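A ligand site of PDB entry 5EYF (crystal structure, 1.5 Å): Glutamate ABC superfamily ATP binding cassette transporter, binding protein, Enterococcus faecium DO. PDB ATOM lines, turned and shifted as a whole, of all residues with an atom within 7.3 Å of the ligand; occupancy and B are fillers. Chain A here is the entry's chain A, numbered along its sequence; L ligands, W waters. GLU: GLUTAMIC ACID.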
ATOM      1  N   LYS A  22     -13.853   2.997  24.559  1.00  0.00           N
ATOM      2  CA  LYS A  22     -13.816   3.593  23.226  1.00  0.00           C
ATOM      3  C   LYS A  22     -12.527   4.390  23.058  1.00  0.00           C
ATOM      4  O   LYS A  22     -11.944   4.885  24.033  1.00  0.00           O
ATOM      5  CB  LYS A  22     -15.008   4.521  22.984  1.00  0.00           C
ATOM      6  CG  LYS A  22     -16.387   3.860  23.226  1.00  0.00           C
ATOM      7  CD  LYS A  22     -16.555   2.652  22.315  1.00  0.00           C
ATOM      8  CE  LYS A  22     -17.979   2.064  22.364  1.00  0.00           C
ATOM      9  NZ  LYS A  22     -18.962   2.875  21.529  1.00  0.00           N
ATOM     10  N   THR A  25     -14.505   8.522  21.155  1.00  0.00           N
ATOM     11  CA  THR A  25     -15.690   9.171  21.736  1.00  0.00           C
ATOM     12  C   THR A  25     -15.233  10.250  22.718  1.00  0.00           C
ATOM     13  O   THR A  25     -14.999   9.991  23.901  1.00  0.00           O
ATOM     14  CB  THR A  25     -16.563   8.127  22.424  1.00  0.00           C
ATOM     15  OG1 THR A  25     -16.902   7.078  21.500  1.00  0.00           O
ATOM     16  CG2 THR A  25     -17.875   8.781  22.994  1.00  0.00           C
ATOM     17  N   THR A  66     -15.101  -1.242  20.131  1.00  0.00           N
ATOM     18  CA  THR A  66     -16.226  -0.540  19.519  1.00  0.00           C
ATOM     19  C   THR A  66     -17.531  -1.139  20.041  1.00  0.00           C
ATOM     20  O   THR A  66     -17.540  -2.150  20.748  1.00  0.00           O
ATOM     21  CB  THR A  66     -16.202  -0.631  17.984  1.00  0.00           C
ATOM     22  OG1 THR A  66     -16.468  -1.983  17.567  1.00  0.00           O
ATOM     23  CG2 THR A  66     -14.839  -0.212  17.418  1.00  0.00           C
ATOM     24  N   SER A  67     -18.642  -0.529  19.649  1.00  0.00           N
ATOM     25  CA  SER A  67     -19.923  -1.110  20.004  1.00  0.00           C
ATOM     26  C   SER A  67     -20.051  -2.512  19.448  1.00  0.00           C
ATOM     27  O   SER A  67     -20.730  -3.365  20.033  1.00  0.00           O
ATOM     28  CB  SER A  67     -21.058  -0.229  19.507  1.00  0.00           C
ATOM     29  OG  SER A  67     -20.976   1.054  20.118  1.00  0.00           O
ATOM     30  N   LYS A  68     -19.401  -2.784  18.318  1.00  0.00           N
ATOM     31  CA  LYS A  68     -19.477  -4.119  17.722  1.00  0.00           C
ATOM     32  C   LYS A  68     -18.570  -5.113  18.424  1.00  0.00           C
ATOM     33  O   LYS A  68     -18.924  -6.284  18.557  1.00  0.00           O
ATOM     34  CB  LYS A  68     -19.090  -4.055  16.236  1.00  0.00           C
ATOM     35  CG  LYS A  68     -20.094  -3.290  15.405  1.00  0.00           C
ATOM     36  CD  LYS A  68     -19.645  -3.142  13.980  1.00  0.00           C
ATOM     37  CE  LYS A  68     -19.137  -4.433  13.400  1.00  0.00           C
ATOM     38  NZ  LYS A  68     -18.711  -4.227  11.991  1.00  0.00           N
ATOM     39  N   ARG A  70     -17.119  -4.984  21.592  1.00  0.00           N
ATOM     40  CA  ARG A  70     -16.922  -4.974  23.037  1.00  0.00           C
ATOM     41  C   ARG A  70     -17.398  -6.280  23.708  1.00  0.00           C
ATOM     42  O   ARG A  70     -16.674  -6.834  24.523  1.00  0.00           O
ATOM     43  CB  ARG A  70     -17.574  -3.735  23.681  1.00  0.00           C
ATOM     44  CG  ARG A  70     -19.089  -3.533  23.494  1.00  0.00           C
ATOM     45  CD  ARG A  70     -19.479  -2.135  23.880  1.00  0.00           C
ATOM     46  NE  ARG A  70     -20.882  -1.956  23.449  1.00  0.00           N
ATOM     47  CZ  ARG A  70     -21.493  -0.760  23.306  1.00  0.00           C
ATOM     48  NH1 ARG A  70     -20.887   0.389  23.677  1.00  0.00           N
ATOM     49  NH2 ARG A  70     -22.704  -0.719  22.811  1.00  0.00           N
ATOM     50  N   ALA A  84     -17.628   1.744  28.212  1.00  0.00           N
ATOM     51  CA  ALA A  84     -17.535   2.199  26.817  1.00  0.00           C
ATOM     52  C   ALA A  84     -18.900   2.652  26.350  1.00  0.00           C
ATOM     53  O   ALA A  84     -19.519   2.024  25.488  1.00  0.00           O
ATOM     54  CB  ALA A  84     -16.993   1.094  25.888  1.00  0.00           C
ATOM     55  N   THR A  85     -19.383   3.750  26.959  1.00  0.00           N
ATOM     56  CA  THR A  85     -20.710   4.351  26.713  1.00  0.00           C
ATOM     57  C   THR A  85     -21.771   3.302  26.438  1.00  0.00           C
ATOM     58  O   THR A  85     -22.508   3.374  25.453  1.00  0.00           O
ATOM     59  CB  THR A  85     -20.663   5.350  25.549  1.00  0.00           C
ATOM     60  OG1 THR A  85     -20.302   4.725  24.305  1.00  0.00           O
ATOM     61  CG2 THR A  85     -19.665   6.444  25.848  1.00  0.00           C
ATOM     62  N   MET A  86     -21.800   2.281  27.314  1.00  0.00           N
ATOM     63  CA  MET A  86     -22.579   1.093  27.033  1.00  0.00           C
ATOM     64  C   MET A  86     -23.873   1.059  27.830  1.00  0.00           C
ATOM     65  O   MET A  86     -23.867   0.882  29.038  1.00  0.00           O
ATOM     66  CB  MET A  86     -21.761  -0.140  27.359  1.00  0.00           C
ATOM     67  CG  MET A  86     -22.434  -1.467  26.866  1.00  0.00           C
ATOM     68  SD  MET A  86     -21.210  -2.907  27.233  1.00  0.00           S
ATOM     69  CE  MET A  86     -22.369  -4.382  26.636  1.00  0.00           C
ATOM     70  N   THR A  87     -24.999   1.157  27.126  1.00  0.00           N
ATOM     71  CA  THR A  87     -26.287   1.098  27.814  1.00  0.00           C
ATOM     72  C   THR A  87     -26.564  -0.286  28.371  1.00  0.00           C
ATOM     73  O   THR A  87     -26.381  -1.309  27.699  1.00  0.00           O
ATOM     74  CB  THR A  87     -27.400   1.488  26.857  1.00  0.00           C
ATOM     75  OG1 THR A  87     -27.114   2.813  26.355  1.00  0.00           O
ATOM     76  CG2 THR A  87     -28.756   1.510  27.572  1.00  0.00           C
ATOM     77  N   ILE A  88     -27.094  -0.306  29.600  1.00  0.00           N
ATOM     78  CA  ILE A  88     -27.626  -1.546  30.189  1.00  0.00           C
ATOM     79  C   ILE A  88     -28.918  -1.894  29.465  1.00  0.00           C
ATOM     80  O   ILE A  88     -29.863  -1.100  29.439  1.00  0.00           O
ATOM     81  CB  ILE A  88     -27.880  -1.363  31.686  1.00  0.00           C
ATOM     82  CG1 ILE A  88     -26.580  -0.923  32.381  1.00  0.00           C
ATOM     83  CG2 ILE A  88     -28.495  -2.678  32.235  1.00  0.00           C
ATOM     84  CD1 ILE A  88     -26.767  -0.752  33.853  1.00  0.00           C
ATOM     85  N   THR A  89     -28.959  -3.057  28.812  1.00  0.00           N
ATOM     86  CA  THR A  89     -30.183  -3.538  28.189  1.00  0.00           C
ATOM     87  C   THR A  89     -30.437  -4.995  28.572  1.00  0.00           C
ATOM     88  O   THR A  89     -29.514  -5.780  28.818  1.00  0.00           O
ATOM     89  CB  THR A  89     -30.191  -3.402  26.649  1.00  0.00           C
ATOM     90  OG1 THR A  89     -29.401  -4.475  26.088  1.00  0.00           O
ATOM     91  CG2 THR A  89     -29.687  -2.021  26.180  1.00  0.00           C
ATOM     92  N   ARG A  92     -28.720  -7.380  26.194  1.00  0.00           N
ATOM     93  CA  ARG A  92     -27.318  -7.610  26.478  1.00  0.00           C
ATOM     94  C   ARG A  92     -27.116  -8.461  27.715  1.00  0.00           C
ATOM     95  O   ARG A  92     -26.109  -9.170  27.802  1.00  0.00           O
ATOM     96  CB  ARG A  92     -26.577  -6.268  26.622  1.00  0.00           C
ATOM     97  CG  ARG A  92     -26.516  -5.515  25.321  1.00  0.00           C
ATOM     98  CD  ARG A  92     -26.091  -4.048  25.467  1.00  0.00           C
ATOM     99  NE  ARG A  92     -26.111  -3.422  24.163  1.00  0.00           N
ATOM    100  CZ  ARG A  92     -25.831  -2.139  23.937  1.00  0.00           C
ATOM    101  NH1 ARG A  92     -25.547  -1.310  24.931  1.00  0.00           N
ATOM    102  NH2 ARG A  92     -25.822  -1.699  22.686  1.00  0.00           N
ATOM    103  N   ALA A 105     -27.529   8.794  30.109  1.00  0.00           N
ATOM    104  CA  ALA A 105     -27.620   9.439  28.791  1.00  0.00           C
ATOM    105  C   ALA A 105     -29.012   9.239  28.181  1.00  0.00           C
ATOM    106  O   ALA A 105     -29.894   8.617  28.786  1.00  0.00           O
ATOM    107  CB  ALA A 105     -26.528   8.886  27.876  1.00  0.00           C
ATOM    108  N   GLN A 107     -30.899   9.178  23.871  1.00  0.00           N
ATOM    109  CA  GLN A 107     -30.657   9.398  22.451  1.00  0.00           C
ATOM    110  C   GLN A 107     -31.176  10.762  22.022  1.00  0.00           C
ATOM    111  O   GLN A 107     -32.240  11.227  22.492  1.00  0.00           O
ATOM    112  CB  GLN A 107     -31.284   8.272  21.621  1.00  0.00           C
ATOM    113  CG  GLN A 107     -30.820   8.360  20.139  1.00  0.00           C
ATOM    114  CD  GLN A 107     -31.175   7.143  19.332  1.00  0.00           C
ATOM    115  OE1 GLN A 107     -31.489   6.085  19.872  1.00  0.00           O
ATOM    116  NE2 GLN A 107     -31.132   7.280  18.017  1.00  0.00           N
ATOM    117  N   SER A 135     -25.910   0.141  15.050  1.00  0.00           N
ATOM    118  CA  SER A 135     -26.059   0.677  16.393  1.00  0.00           C
ATOM    119  C   SER A 135     -27.497   0.566  16.884  1.00  0.00           C
ATOM    120  O   SER A 135     -28.462   0.523  16.104  1.00  0.00           O
ATOM    121  CB  SER A 135     -25.637   2.158  16.446  1.00  0.00           C
ATOM    122  OG  SER A 135     -26.483   2.991  15.639  1.00  0.00           O
ATOM    123  N   THR A 136     -27.620   0.602  18.203  1.00  0.00           N
ATOM    124  CA  THR A 136     -28.941   0.735  18.798  1.00  0.00           C
ATOM    125  C   THR A 136     -29.586   2.034  18.358  1.00  0.00           C
ATOM    126  O   THR A 136     -30.793   2.077  18.115  1.00  0.00           O
ATOM    127  CB  THR A 136     -28.864   0.724  20.322  1.00  0.00           C
ATOM    128  OG1 THR A 136     -28.001   1.786  20.755  1.00  0.00           O
ATOM    129  CG2 THR A 136     -28.391  -0.658  20.826  1.00  0.00           C
ATOM    130  N   SER A 137     -28.764   3.079  18.182  1.00  0.00           N
ATOM    131  CA  SER A 137     -29.274   4.378  17.763  1.00  0.00           C
ATOM    132  C   SER A 137     -29.984   4.291  16.431  1.00  0.00           C
ATOM    133  O   SER A 137     -31.040   4.915  16.234  1.00  0.00           O
ATOM    134  CB  SER A 137     -28.113   5.370  17.656  1.00  0.00           C
ATOM    135  OG  SER A 137     -27.226   5.264  18.779  1.00  0.00           O
ATOM    136  N   ASN A 140     -33.277   2.532  16.933  1.00  0.00           N
ATOM    137  CA  ASN A 140     -34.239   3.346  17.668  1.00  0.00           C
ATOM    138  C   ASN A 140     -34.822   4.419  16.794  1.00  0.00           C
ATOM    139  O   ASN A 140     -36.022   4.717  16.894  1.00  0.00           O
ATOM    140  CB  ASN A 140     -33.595   3.985  18.888  1.00  0.00           C
ATOM    141  CG  ASN A 140     -33.277   2.982  19.972  1.00  0.00           C
ATOM    142  OD1 ASN A 140     -33.905   1.907  20.051  1.00  0.00           O
ATOM    143  ND2 ASN A 140     -32.339   3.321  20.834  1.00  0.00           N
ATOM    144  N   TYR A 156     -18.741   7.410  14.237  1.00  0.00           N
ATOM    145  CA  TYR A 156     -19.183   8.771  14.509  1.00  0.00           C
ATOM    146  C   TYR A 156     -18.514   9.774  13.600  1.00  0.00           C
ATOM    147  O   TYR A 156     -19.146  10.740  13.160  1.00  0.00           O
ATOM    148  CB  TYR A 156     -18.905   9.176  15.954  1.00  0.00           C
ATOM    149  CG  TYR A 156     -19.492   8.271  16.998  1.00  0.00           C
ATOM    150  CD1 TYR A 156     -20.832   7.900  16.966  1.00  0.00           C
ATOM    151  CD2 TYR A 156     -18.698   7.767  18.025  1.00  0.00           C
ATOM    152  CE1 TYR A 156     -21.354   7.058  17.953  1.00  0.00           C
ATOM    153  CE2 TYR A 156     -19.211   6.946  18.983  1.00  0.00           C
ATOM    154  CZ  TYR A 156     -20.540   6.604  18.945  1.00  0.00           C
ATOM    155  OH  TYR A 156     -21.058   5.749  19.927  1.00  0.00           O
ATOM    156  N   THR A 173     -27.148   9.920  18.059  1.00  0.00           N
ATOM    157  CA  THR A 173     -26.578   8.943  18.979  1.00  0.00           C
ATOM    158  C   THR A 173     -26.834   9.512  20.369  1.00  0.00           C
ATOM    159  O   THR A 173     -27.723  10.355  20.527  1.00  0.00           O
ATOM    160  CB  THR A 173     -25.093   8.665  18.691  1.00  0.00           C
ATOM    161  OG1 THR A 173     -24.590   7.710  19.651  1.00  0.00           O
ATOM    162  CG2 THR A 173     -24.236   9.941  18.742  1.00  0.00           C
ATOM    163  N   ASP A 174     -26.152   9.048  21.403  1.00  0.00           N
ATOM    164  CA  ASP A 174     -26.448   9.529  22.755  1.00  0.00           C
ATOM    165  C   ASP A 174     -26.150  11.015  22.874  1.00  0.00           C
ATOM    166  O   ASP A 174     -25.167  11.503  22.314  1.00  0.00           O
ATOM    167  CB  ASP A 174     -25.624   8.784  23.796  1.00  0.00           C
ATOM    168  CG  ASP A 174     -25.925   7.290  23.853  1.00  0.00           C
ATOM    169  OD1 ASP A 174     -26.959   6.830  23.293  1.00  0.00           O
ATOM    170  OD2 ASP A 174     -25.128   6.593  24.543  1.00  0.00           O
ATOM    171  N   ILE A 177     -22.587  11.955  23.883  1.00  0.00           N
ATOM    172  CA  ILE A 177     -21.639  11.761  22.799  1.00  0.00           C
ATOM    173  C   ILE A 177     -21.743  12.908  21.799  1.00  0.00           C
ATOM    174  O   ILE A 177     -20.733  13.460  21.350  1.00  0.00           O
ATOM    175  CB  ILE A 177     -21.897  10.386  22.153  1.00  0.00           C
ATOM    176  CG1 ILE A 177     -21.643   9.287  23.184  1.00  0.00           C
ATOM    177  CG2 ILE A 177     -21.048  10.203  20.885  1.00  0.00           C
ATOM    178  CD1 ILE A 177     -21.940   7.889  22.630  1.00  0.00           C
ATOM    179  N   GLU A 198     -30.672   6.009  28.153  1.00  0.00           N
ATOM    180  CA  GLU A 198     -29.457   5.234  27.886  1.00  0.00           C
ATOM    181  C   GLU A 198     -28.620   5.197  29.158  1.00  0.00           C
ATOM    182  O   GLU A 198     -27.626   5.922  29.264  1.00  0.00           O
ATOM    183  CB  GLU A 198     -28.655   5.821  26.713  1.00  0.00           C
ATOM    184  CG  GLU A 198     -29.443   5.958  25.435  1.00  0.00           C
ATOM    185  CD  GLU A 198     -29.798   4.645  24.752  1.00  0.00           C
ATOM    186  OE1 GLU A 198     -29.106   3.608  24.918  1.00  0.00           O
ATOM    187  OE2 GLU A 198     -30.808   4.646  24.012  1.00  0.00           O
ATOM    188  N   PRO A 199     -29.026   4.413  30.169  1.00  0.00           N
ATOM    189  CA  PRO A 199     -28.219   4.329  31.403  1.00  0.00           C
ATOM    190  C   PRO A 199     -26.965   3.508  31.140  1.00  0.00           C
ATOM    191  O   PRO A 199     -27.065   2.366  30.691  1.00  0.00           O
ATOM    192  CB  PRO A 199     -29.158   3.644  32.403  1.00  0.00           C
ATOM    193  CG  PRO A 199     -30.079   2.814  31.490  1.00  0.00           C
ATOM    194  CD  PRO A 199     -30.300   3.662  30.269  1.00  0.00           C
ATOM    195  N   TYR A 200     -25.787   4.088  31.370  1.00  0.00           N
ATOM    196  CA  TYR A 200     -24.534   3.361  31.105  1.00  0.00           C
ATOM    197  C   TYR A 200     -24.187   2.479  32.295  1.00  0.00           C
ATOM    198  O   TYR A 200     -24.276   2.898  33.460  1.00  0.00           O
ATOM    199  CB  TYR A 200     -23.393   4.318  30.894  1.00  0.00           C
ATOM    200  CG  TYR A 200     -23.457   5.193  29.662  1.00  0.00           C
ATOM    201  CD1 TYR A 200     -24.457   5.031  28.691  1.00  0.00           C
ATOM    202  CD2 TYR A 200     -22.516   6.203  29.491  1.00  0.00           C
ATOM    203  CE1 TYR A 200     -24.453   5.859  27.520  1.00  0.00           C
ATOM    204  CE2 TYR A 200     -22.537   7.027  28.372  1.00  0.00           C
ATOM    205  CZ  TYR A 200     -23.504   6.868  27.412  1.00  0.00           C
ATOM    206  OH  TYR A 200     -23.507   7.681  26.294  1.00  0.00           O
HETATM  207  N   GLU L   1     -25.186   3.891  24.586  1.00  0.00           N
HETATM  208  CA  GLU L   1     -25.718   3.317  23.349  1.00  0.00           C
HETATM  209  C   GLU L   1     -25.495   1.817  23.350  1.00  0.00           C
HETATM  210  O   GLU L   1     -24.762   1.310  24.210  1.00  0.00           O
HETATM  211  CB  GLU L   1     -25.087   3.967  22.089  1.00  0.00           C
HETATM  212  CG  GLU L   1     -23.572   4.232  22.161  1.00  0.00           C
HETATM  213  CD  GLU L   1     -22.717   2.957  21.988  1.00  0.00           C
HETATM  214  OE1 GLU L   1     -21.602   2.952  22.549  1.00  0.00           O
HETATM  215  OE2 GLU L   1     -23.169   1.975  21.332  1.00  0.00           O
HETATM  216  OXT GLU L   1     -26.077   1.136  22.470  1.00  0.00           O
HETATM  217  O   HOH W   1     -22.520   3.607  18.526  1.00  0.00           O
HETATM  218  O   HOH W   2     -29.269   1.172  23.859  1.00  0.00           O
HETATM  219  O   HOH W   3     -24.983   0.602  19.588  1.00  0.00           O
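Residues that only touch the ligand: Met 86, Tyr 200, Tyr 156 and Ala 84. Hydrophobic or aromatic side chains within 4 Å of the ligand: Tyr 200. 13 residues have an atom within 4 Å of the ligand: Lys 22, Ser 67, Arg 70, Ala 84, Thr 85, Met 86, Thr 87, Arg 92, Thr 136, Tyr 156, Asp 174, Glu 198 and Tyr 200.
The side-chain hydroxyl (OG1) of Thr 136 lies within hydrogen-bond range of an oxygen (OXT) of the ligand (2.7 Å). OG of Ser 67 sits at hydrogen-bond distance from OE2 of the ligand (2.7 Å). The side-chain carboxylate of Asp 174 lies within salt-bridge range of a nitrogen (N) of the ligand, 2.7 Å away. The backbone carbonyl oxygen (O) of Thr 85 lies within hydrogen-bond range of a nitrogen (N) of the ligand, 2.9 Å away. An oxygen (OE1) of the ligand lies within hydrogen-bond range of the side-chain hydroxyl (OG1) of Thr 85 (2.8 Å). NH1 of Arg 92 is in salt-bridge range of O of the ligand, at 2.8 Å. The backbone NH of Thr 87 sits at hydrogen-bond distance from an oxygen (O) of the ligand (2.9 Å). A nitrogen (N) of the ligand sits at hydrogen-bond distance from the side-chain hydroxyl (OG1) of Thr 87 (2.8 Å). An oxygen (OE1) of the ligand is in salt-bridge range of the side-chain amino group of Lys 22. NH1 of Arg 70 lies within salt-bridge range of OE1 of the ligand, at 2.9 Å. The side-chain carboxylate (OE1) of Glu 198 is in salt-bridge range of a nitrogen (N) of the ligand (3.9 Å).
ND2 of Asn 140 sits close to O of Thr 136, 3.4 Å away. The side-chain hydroxyl (OG) of Ser 67 is in hydrogen-bond range of the side-chain amino group (NZ) of Lys 22 (3.1 Å). OH of Tyr 200 sits at hydrogen-bond distance from OD2 of Asp 174. The guanidinium group (NH1) of Arg 92 sits at hydrogen-bond distance from the backbone carbonyl oxygen (O) of Thr 87, 2.9 Å away. OG1 of Thr 89 sits at hydrogen-bond distance from N of Arg 92 (3.0 Å). The side-chain hydroxyl of Thr 87 is in hydrogen-bond range of the side-chain carboxylate of Glu 198 (2.6 Å). The guanidinium group (NH1) of Arg 70 is in hydrogen-bond range of the backbone carbonyl oxygen (O) of Ala 84 (2.8 Å). O of Ala 105 sits at hydrogen-bond distance from N of Glu 198 (2.8 Å).
Water W3 lies within hydrogen-bond range of an oxygen (OE2) of the ligand (2.9 Å) and the backbone NH (N) of Thr 136 (3.0 Å). Water W1 lies within hydrogen-bond range of the side-chain hydroxyl (OH) of Tyr 156, an oxygen (OE2) of the ligand and the side-chain hydroxyl (OG) of Ser 67. Water W2 lies within hydrogen-bond range of OE1 of Glu 198 (2.7 Å), OG1 of Thr 136 (3.4 Å) and OXT of the ligand (3.5 Å).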
